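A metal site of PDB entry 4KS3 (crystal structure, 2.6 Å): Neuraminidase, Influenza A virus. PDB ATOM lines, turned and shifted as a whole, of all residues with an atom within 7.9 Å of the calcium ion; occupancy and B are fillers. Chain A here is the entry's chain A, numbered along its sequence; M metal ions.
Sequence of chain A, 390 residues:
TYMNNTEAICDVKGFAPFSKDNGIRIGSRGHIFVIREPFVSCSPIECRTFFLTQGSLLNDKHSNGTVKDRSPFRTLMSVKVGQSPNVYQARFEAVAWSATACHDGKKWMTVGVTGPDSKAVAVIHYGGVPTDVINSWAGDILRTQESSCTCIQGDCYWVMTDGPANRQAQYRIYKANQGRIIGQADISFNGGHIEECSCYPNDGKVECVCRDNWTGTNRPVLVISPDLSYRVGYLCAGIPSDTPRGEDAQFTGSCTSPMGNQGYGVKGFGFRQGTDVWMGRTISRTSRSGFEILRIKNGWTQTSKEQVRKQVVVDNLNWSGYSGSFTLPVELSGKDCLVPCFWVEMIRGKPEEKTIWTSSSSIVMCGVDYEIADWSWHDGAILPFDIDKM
The backbone NH of Gly 216 sits at hydrogen-bond distance from the side-chain carboxylate of Asp 212.
The side-chain carboxylate of Asp 212 is in hydrogen-bond range of the backbone NH of Trp 214.
The backbone NH (N) of Asp 242 is in hydrogen-bond range of the backbone carbonyl oxygen (O) of Thr 217.
The side-chain carboxylate (OD2) of Asp 242 is in hydrogen-bond range of the backbone NH (N) of Val 266 (2.9 Å).
The guanidinium group (NH2) of Arg 245 sits at hydrogen-bond distance from the backbone carbonyl oxygen (O) of Asp 242 (2.9 Å).
The guanidinium group (NH1) of Arg 219 lies within salt-bridge range of the side-chain carboxylate (OD2) of Asp 242, 3.8 Å away.
OD1 of Asn 213 lies within hydrogen-bond range of N of Gly 265 (3.2 Å).
NH1 of Arg 211 lies within hydrogen-bond range of O of Gly 265 (2.7 Å).
Merely in contact with the calcium ion: Gly 263 and Gly 265.
Within 4 Å of the calcium ion: Asp 212, Gly 216, Asp 242, Gly 263, Tyr 264 and Gly 265.
The nearest printed residue that does not touch the calcium ion is Asn 213 (4.2 Å).
O of Asp 212 is bound to the calcium ion, 2.2 Å away.
O of Tyr 264 is bound to the calcium ion, at 2.2 Å.
OD1 of Asp 242 binds the calcium ion (2.4 Å).
O of Gly 216 binds the calcium ion (2.7 Å).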
ATOM      1  N   HIS A 193      33.898 -21.530 -25.814  1.00  0.00           N
ATOM      2  CA  HIS A 193      32.634 -22.242 -25.646  1.00  0.00           C
ATOM      3  C   HIS A 193      31.468 -21.631 -26.430  1.00  0.00           C
ATOM      4  O   HIS A 193      30.968 -20.547 -26.098  1.00  0.00           O
ATOM      5  CB  HIS A 193      32.272 -22.342 -24.159  1.00  0.00           C
ATOM      6  CG  HIS A 193      31.270 -23.413 -23.855  1.00  0.00           C
ATOM      7  ND1 HIS A 193      30.004 -23.436 -24.411  1.00  0.00           N
ATOM      8  CD2 HIS A 193      31.342 -24.513 -23.057  1.00  0.00           C
ATOM      9  CE1 HIS A 193      29.352 -24.502 -23.968  1.00  0.00           C
ATOM     10  NE2 HIS A 193      30.140 -25.171 -23.148  1.00  0.00           N
ATOM     11  N   ARG A 211      26.543 -18.410 -27.565  1.00  0.00           N
ATOM     12  CA  ARG A 211      26.598 -18.313 -26.108  1.00  0.00           C
ATOM     13  C   ARG A 211      27.749 -19.056 -25.480  1.00  0.00           C
ATOM     14  O   ARG A 211      28.028 -20.189 -25.853  1.00  0.00           O
ATOM     15  CB  ARG A 211      25.281 -18.852 -25.559  1.00  0.00           C
ATOM     16  CG  ARG A 211      25.316 -19.271 -24.090  1.00  0.00           C
ATOM     17  CD  ARG A 211      24.001 -19.946 -23.723  1.00  0.00           C
ATOM     18  NE  ARG A 211      23.898 -20.326 -22.324  1.00  0.00           N
ATOM     19  CZ  ARG A 211      22.793 -20.835 -21.770  1.00  0.00           C
ATOM     20  NH1 ARG A 211      22.780 -21.154 -20.484  1.00  0.00           N
ATOM     21  NH2 ARG A 211      21.699 -21.012 -22.501  1.00  0.00           N
ATOM     22  N   ASP A 212      28.426 -18.412 -24.542  1.00  0.00           N
ATOM     23  CA  ASP A 212      29.511 -19.035 -23.805  1.00  0.00           C
ATOM     24  C   ASP A 212      28.974 -19.479 -22.450  1.00  0.00           C
ATOM     25  O   ASP A 212      28.707 -18.659 -21.582  1.00  0.00           O
ATOM     26  CB  ASP A 212      30.669 -18.033 -23.617  1.00  0.00           C
ATOM     27  CG  ASP A 212      31.977 -18.697 -23.153  1.00  0.00           C
ATOM     28  OD1 ASP A 212      33.058 -18.113 -23.412  1.00  0.00           O
ATOM     29  OD2 ASP A 212      31.934 -19.770 -22.514  1.00  0.00           O
ATOM     30  N   ASN A 213      28.811 -20.772 -22.271  1.00  0.00           N
ATOM     31  CA  ASN A 213      28.314 -21.269 -21.005  1.00  0.00           C
ATOM     32  C   ASN A 213      29.460 -21.685 -20.091  1.00  0.00           C
ATOM     33  O   ASN A 213      29.250 -22.237 -19.016  1.00  0.00           O
ATOM     34  CB  ASN A 213      27.338 -22.412 -21.236  1.00  0.00           C
ATOM     35  CG  ASN A 213      26.192 -22.410 -20.240  1.00  0.00           C
ATOM     36  OD1 ASN A 213      25.276 -21.594 -20.358  1.00  0.00           O
ATOM     37  ND2 ASN A 213      26.245 -23.304 -19.269  1.00  0.00           N
ATOM     38  N   TRP A 214      30.680 -21.381 -20.506  1.00  0.00           N
ATOM     39  CA  TRP A 214      31.835 -21.771 -19.722  1.00  0.00           C
ATOM     40  C   TRP A 214      32.270 -20.661 -18.777  1.00  0.00           C
ATOM     41  O   TRP A 214      31.935 -20.679 -17.588  1.00  0.00           O
ATOM     42  CB  TRP A 214      32.997 -22.199 -20.633  1.00  0.00           C
ATOM     43  CG  TRP A 214      34.061 -22.979 -19.930  1.00  0.00           C
ATOM     44  CD1 TRP A 214      34.094 -23.310 -18.599  1.00  0.00           C
ATOM     45  CD2 TRP A 214      35.239 -23.537 -20.503  1.00  0.00           C
ATOM     46  NE1 TRP A 214      35.226 -24.022 -18.320  1.00  0.00           N
ATOM     47  CE2 TRP A 214      35.951 -24.179 -19.472  1.00  0.00           C
ATOM     48  CE3 TRP A 214      35.777 -23.540 -21.789  1.00  0.00           C
ATOM     49  CZ2 TRP A 214      37.165 -24.824 -19.686  1.00  0.00           C
ATOM     50  CZ3 TRP A 214      36.974 -24.173 -21.997  1.00  0.00           C
ATOM     51  CH2 TRP A 214      37.659 -24.812 -20.953  1.00  0.00           C
ATOM     52  N   THR A 215      33.020 -19.687 -19.295  1.00  0.00           N
ATOM     53  CA  THR A 215      33.500 -18.575 -18.493  1.00  0.00           C
ATOM     54  C   THR A 215      33.141 -17.203 -19.043  1.00  0.00           C
ATOM     55  O   THR A 215      32.849 -16.286 -18.288  1.00  0.00           O
ATOM     56  CB  THR A 215      35.037 -18.609 -18.311  1.00  0.00           C
ATOM     57  OG1 THR A 215      35.682 -18.643 -19.600  1.00  0.00           O
ATOM     58  CG2 THR A 215      35.478 -19.815 -17.476  1.00  0.00           C
ATOM     59  N   GLY A 216      33.159 -17.060 -20.368  1.00  0.00           N
ATOM     60  CA  GLY A 216      32.911 -15.778 -20.989  1.00  0.00           C
ATOM     61  C   GLY A 216      31.577 -15.133 -20.654  1.00  0.00           C
ATOM     62  O   GLY A 216      30.539 -15.799 -20.674  1.00  0.00           O
ATOM     63  N   THR A 217      31.608 -13.841 -20.338  1.00  0.00           N
ATOM     64  CA  THR A 217      30.377 -13.054 -20.229  1.00  0.00           C
ATOM     65  C   THR A 217      30.228 -12.200 -21.475  1.00  0.00           C
ATOM     66  O   THR A 217      29.270 -11.437 -21.612  1.00  0.00           O
ATOM     67  CB  THR A 217      30.364 -12.187 -18.973  1.00  0.00           C
ATOM     68  OG1 THR A 217      31.573 -11.420 -18.911  1.00  0.00           O
ATOM     69  CG2 THR A 217      30.278 -13.052 -17.736  1.00  0.00           C
ATOM     70  N   ASN A 218      31.193 -12.328 -22.382  1.00  0.00           N
ATOM     71  CA  ASN A 218      31.029 -11.865 -23.759  1.00  0.00           C
ATOM     72  C   ASN A 218      30.656 -13.053 -24.621  1.00  0.00           C
ATOM     73  O   ASN A 218      30.724 -14.199 -24.177  1.00  0.00           O
ATOM     74  CB  ASN A 218      32.310 -11.233 -24.268  1.00  0.00           C
ATOM     75  CG  ASN A 218      33.506 -12.125 -24.072  1.00  0.00           C
ATOM     76  OD1 ASN A 218      33.507 -12.975 -23.186  1.00  0.00           O
ATOM     77  ND2 ASN A 218      34.534 -11.945 -24.906  1.00  0.00           N
ATOM     78  N   ARG A 219      30.253 -12.789 -25.872  1.00  0.00           N
ATOM     79  CA  ARG A 219      29.686 -13.828 -26.724  1.00  0.00           C
ATOM     80  C   ARG A 219      30.600 -14.243 -27.866  1.00  0.00           C
ATOM     81  O   ARG A 219      31.122 -13.398 -28.594  1.00  0.00           O
ATOM     82  CB  ARG A 219      28.317 -13.392 -27.263  1.00  0.00           C
ATOM     83  CG  ARG A 219      27.261 -13.144 -26.192  1.00  0.00           C
ATOM     84  CD  ARG A 219      25.856 -13.014 -26.795  1.00  0.00           C
ATOM     85  NE  ARG A 219      24.825 -12.824 -25.765  1.00  0.00           N
ATOM     86  CZ  ARG A 219      24.159 -13.803 -25.159  1.00  0.00           C
ATOM     87  NH1 ARG A 219      23.239 -13.528 -24.244  1.00  0.00           N
ATOM     88  NH2 ARG A 219      24.415 -15.072 -25.470  1.00  0.00           N
ATOM     89  N   PRO A 220      30.801 -15.571 -28.032  1.00  0.00           N
ATOM     90  CA  PRO A 220      31.551 -16.112 -29.164  1.00  0.00           C
ATOM     91  C   PRO A 220      31.032 -15.583 -30.495  1.00  0.00           C
ATOM     92  O   PRO A 220      29.853 -15.308 -30.626  1.00  0.00           O
ATOM     93  CB  PRO A 220      31.295 -17.629 -29.080  1.00  0.00           C
ATOM     94  CG  PRO A 220      30.337 -17.824 -27.942  1.00  0.00           C
ATOM     95  CD  PRO A 220      30.427 -16.624 -27.082  1.00  0.00           C
ATOM     96  N   SER A 241      27.508  -9.082 -22.832  1.00  0.00           N
ATOM     97  CA  SER A 241      26.128  -9.191 -23.264  1.00  0.00           C
ATOM     98  C   SER A 241      25.520 -10.554 -22.976  1.00  0.00           C
ATOM     99  O   SER A 241      24.427 -10.865 -23.437  1.00  0.00           O
ATOM    100  CB  SER A 241      25.983  -8.839 -24.742  1.00  0.00           C
ATOM    101  OG  SER A 241      26.398  -9.895 -25.570  1.00  0.00           O
ATOM    102  N   ASP A 242      26.229 -11.371 -22.196  1.00  0.00           N
ATOM    103  CA  ASP A 242      25.663 -12.617 -21.693  1.00  0.00           C
ATOM    104  C   ASP A 242      24.821 -12.314 -20.467  1.00  0.00           C
ATOM    105  O   ASP A 242      24.609 -11.152 -20.102  1.00  0.00           O
ATOM    106  CB  ASP A 242      26.778 -13.608 -21.334  1.00  0.00           C
ATOM    107  CG  ASP A 242      26.381 -15.068 -21.549  1.00  0.00           C
ATOM    108  OD1 ASP A 242      27.278 -15.924 -21.692  1.00  0.00           O
ATOM    109  OD2 ASP A 242      25.175 -15.373 -21.581  1.00  0.00           O
ATOM    110  N   THR A 243      24.324 -13.350 -19.816  1.00  0.00           N
ATOM    111  CA  THR A 243      23.664 -13.210 -18.531  1.00  0.00           C
ATOM    112  C   THR A 243      23.833 -14.538 -17.791  1.00  0.00           C
ATOM    113  O   THR A 243      23.456 -15.587 -18.324  1.00  0.00           O
ATOM    114  CB  THR A 243      22.174 -12.896 -18.678  1.00  0.00           C
ATOM    115  OG1 THR A 243      22.009 -11.714 -19.463  1.00  0.00           O
ATOM    116  CG2 THR A 243      21.535 -12.681 -17.315  1.00  0.00           C
ATOM    117  N   PRO A 244      24.417 -14.509 -16.580  1.00  0.00           N
ATOM    118  CA  PRO A 244      24.911 -13.340 -15.863  1.00  0.00           C
ATOM    119  C   PRO A 244      26.275 -12.837 -16.338  1.00  0.00           C
ATOM    120  O   PRO A 244      27.081 -13.578 -16.908  1.00  0.00           O
ATOM    121  CB  PRO A 244      25.036 -13.848 -14.418  1.00  0.00           C
ATOM    122  CG  PRO A 244      25.329 -15.282 -14.567  1.00  0.00           C
ATOM    123  CD  PRO A 244      24.588 -15.747 -15.799  1.00  0.00           C
ATOM    124  N   ARG A 245      26.519 -11.560 -16.085  1.00  0.00           N
ATOM    125  CA  ARG A 245      27.740 -10.893 -16.481  1.00  0.00           C
ATOM    126  C   ARG A 245      28.054  -9.954 -15.339  1.00  0.00           C
ATOM    127  O   ARG A 245      27.289  -9.858 -14.374  1.00  0.00           O
ATOM    128  CB  ARG A 245      27.484 -10.071 -17.732  1.00  0.00           C
ATOM    129  CG  ARG A 245      26.375  -9.038 -17.508  1.00  0.00           C
ATOM    130  CD  ARG A 245      25.976  -8.254 -18.743  1.00  0.00           C
ATOM    131  NE  ARG A 245      24.868  -7.354 -18.438  1.00  0.00           N
ATOM    132  CZ  ARG A 245      23.581  -7.683 -18.561  1.00  0.00           C
ATOM    133  NH1 ARG A 245      22.649  -6.794 -18.246  1.00  0.00           N
ATOM    134  NH2 ARG A 245      23.233  -8.878 -19.006  1.00  0.00           N
ATOM    135  N   MET A 259      35.817 -13.531 -21.585  1.00  0.00           N
ATOM    136  CA  MET A 259      36.036 -12.553 -20.530  1.00  0.00           C
ATOM    137  C   MET A 259      34.946 -12.578 -19.468  1.00  0.00           C
ATOM    138  O   MET A 259      33.774 -12.782 -19.752  1.00  0.00           O
ATOM    139  CB  MET A 259      36.193 -11.151 -21.120  1.00  0.00           C
ATOM    140  CG  MET A 259      37.460 -10.954 -21.942  1.00  0.00           C
ATOM    141  SD  MET A 259      38.959 -11.144 -20.959  1.00  0.00           S
ATOM    142  CE  MET A 259      38.532 -10.223 -19.487  1.00  0.00           C
ATOM    143  N   GLY A 260      35.363 -12.333 -18.232  1.00  0.00           N
ATOM    144  CA  GLY A 260      34.521 -12.545 -17.082  1.00  0.00           C
ATOM    145  C   GLY A 260      34.793 -13.926 -16.537  1.00  0.00           C
ATOM    146  O   GLY A 260      35.251 -14.814 -17.260  1.00  0.00           O
ATOM    147  N   ASN A 261      34.539 -14.120 -15.249  1.00  0.00           N
ATOM    148  CA  ASN A 261      34.568 -15.451 -14.679  1.00  0.00           C
ATOM    149  C   ASN A 261      33.243 -15.820 -14.029  1.00  0.00           C
ATOM    150  O   ASN A 261      33.202 -16.336 -12.910  1.00  0.00           O
ATOM    151  CB  ASN A 261      35.732 -15.613 -13.700  1.00  0.00           C
ATOM    152  CG  ASN A 261      37.066 -15.652 -14.411  1.00  0.00           C
ATOM    153  OD1 ASN A 261      37.138 -15.731 -15.638  1.00  0.00           O
ATOM    154  ND2 ASN A 261      38.135 -15.631 -13.631  1.00  0.00           N
ATOM    155  N   GLN A 262      32.160 -15.512 -14.736  1.00  0.00           N
ATOM    156  CA  GLN A 262      30.854 -15.988 -14.356  1.00  0.00           C
ATOM    157  C   GLN A 262      30.517 -17.185 -15.238  1.00  0.00           C
ATOM    158  O   GLN A 262      30.746 -17.155 -16.448  1.00  0.00           O
ATOM    159  CB  GLN A 262      29.818 -14.885 -14.574  1.00  0.00           C
ATOM    160  CG  GLN A 262      30.302 -13.490 -14.214  1.00  0.00           C
ATOM    161  CD  GLN A 262      29.636 -12.949 -12.971  1.00  0.00           C
ATOM    162  OE1 GLN A 262      29.312 -13.701 -12.047  1.00  0.00           O
ATOM    163  NE2 GLN A 262      29.406 -11.642 -12.943  1.00  0.00           N
ATOM    164  N   GLY A 263      29.983 -18.229 -14.631  1.00  0.00           N
ATOM    165  CA  GLY A 263      29.575 -19.400 -15.385  1.00  0.00           C
ATOM    166  C   GLY A 263      28.261 -19.125 -16.082  1.00  0.00           C
ATOM    167  O   GLY A 263      27.859 -17.982 -16.219  1.00  0.00           O
ATOM    168  N   TYR A 264      27.617 -20.193 -16.562  1.00  0.00           N
ATOM    169  CA  TYR A 264      26.264 -20.092 -17.089  1.00  0.00           C
ATOM    170  C   TYR A 264      26.195 -19.228 -18.353  1.00  0.00           C
ATOM    171  O   TYR A 264      27.210 -18.935 -18.989  1.00  0.00           O
ATOM    172  CB  TYR A 264      25.341 -19.545 -15.999  1.00  0.00           C
ATOM    173  CG  TYR A 264      23.859 -19.539 -16.303  1.00  0.00           C
ATOM    174  CD1 TYR A 264      23.348 -20.217 -17.404  1.00  0.00           C
ATOM    175  CD2 TYR A 264      22.972 -18.861 -15.481  1.00  0.00           C
ATOM    176  CE1 TYR A 264      21.981 -20.209 -17.672  1.00  0.00           C
ATOM    177  CE2 TYR A 264      21.616 -18.852 -15.736  1.00  0.00           C
ATOM    178  CZ  TYR A 264      21.127 -19.521 -16.840  1.00  0.00           C
ATOM    179  OH  TYR A 264      19.774 -19.505 -17.083  1.00  0.00           O
ATOM    180  N   GLY A 265      24.984 -18.825 -18.700  1.00  0.00           N
ATOM    181  CA  GLY A 265      24.761 -18.006 -19.867  1.00  0.00           C
ATOM    182  C   GLY A 265      23.300 -17.969 -20.267  1.00  0.00           C
ATOM    183  O   GLY A 265      22.441 -18.593 -19.639  1.00  0.00           O
ATOM    184  N   VAL A 266      23.012 -17.229 -21.326  1.00  0.00           N
ATOM    185  CA  VAL A 266      21.687 -17.206 -21.917  1.00  0.00           C
ATOM    186  C   VAL A 266      21.859 -16.935 -23.391  1.00  0.00           C
ATOM    187  O   VAL A 266      22.844 -16.333 -23.824  1.00  0.00           O
ATOM    188  CB  VAL A 266      20.778 -16.147 -21.271  1.00  0.00           C
ATOM    189  CG1 VAL A 266      21.155 -14.764 -21.775  1.00  0.00           C
ATOM    190  CG2 VAL A 266      19.313 -16.446 -21.571  1.00  0.00           C
HETATM  191 CA    CA M   1      28.329 -17.248 -19.927  1.00  0.00          CA
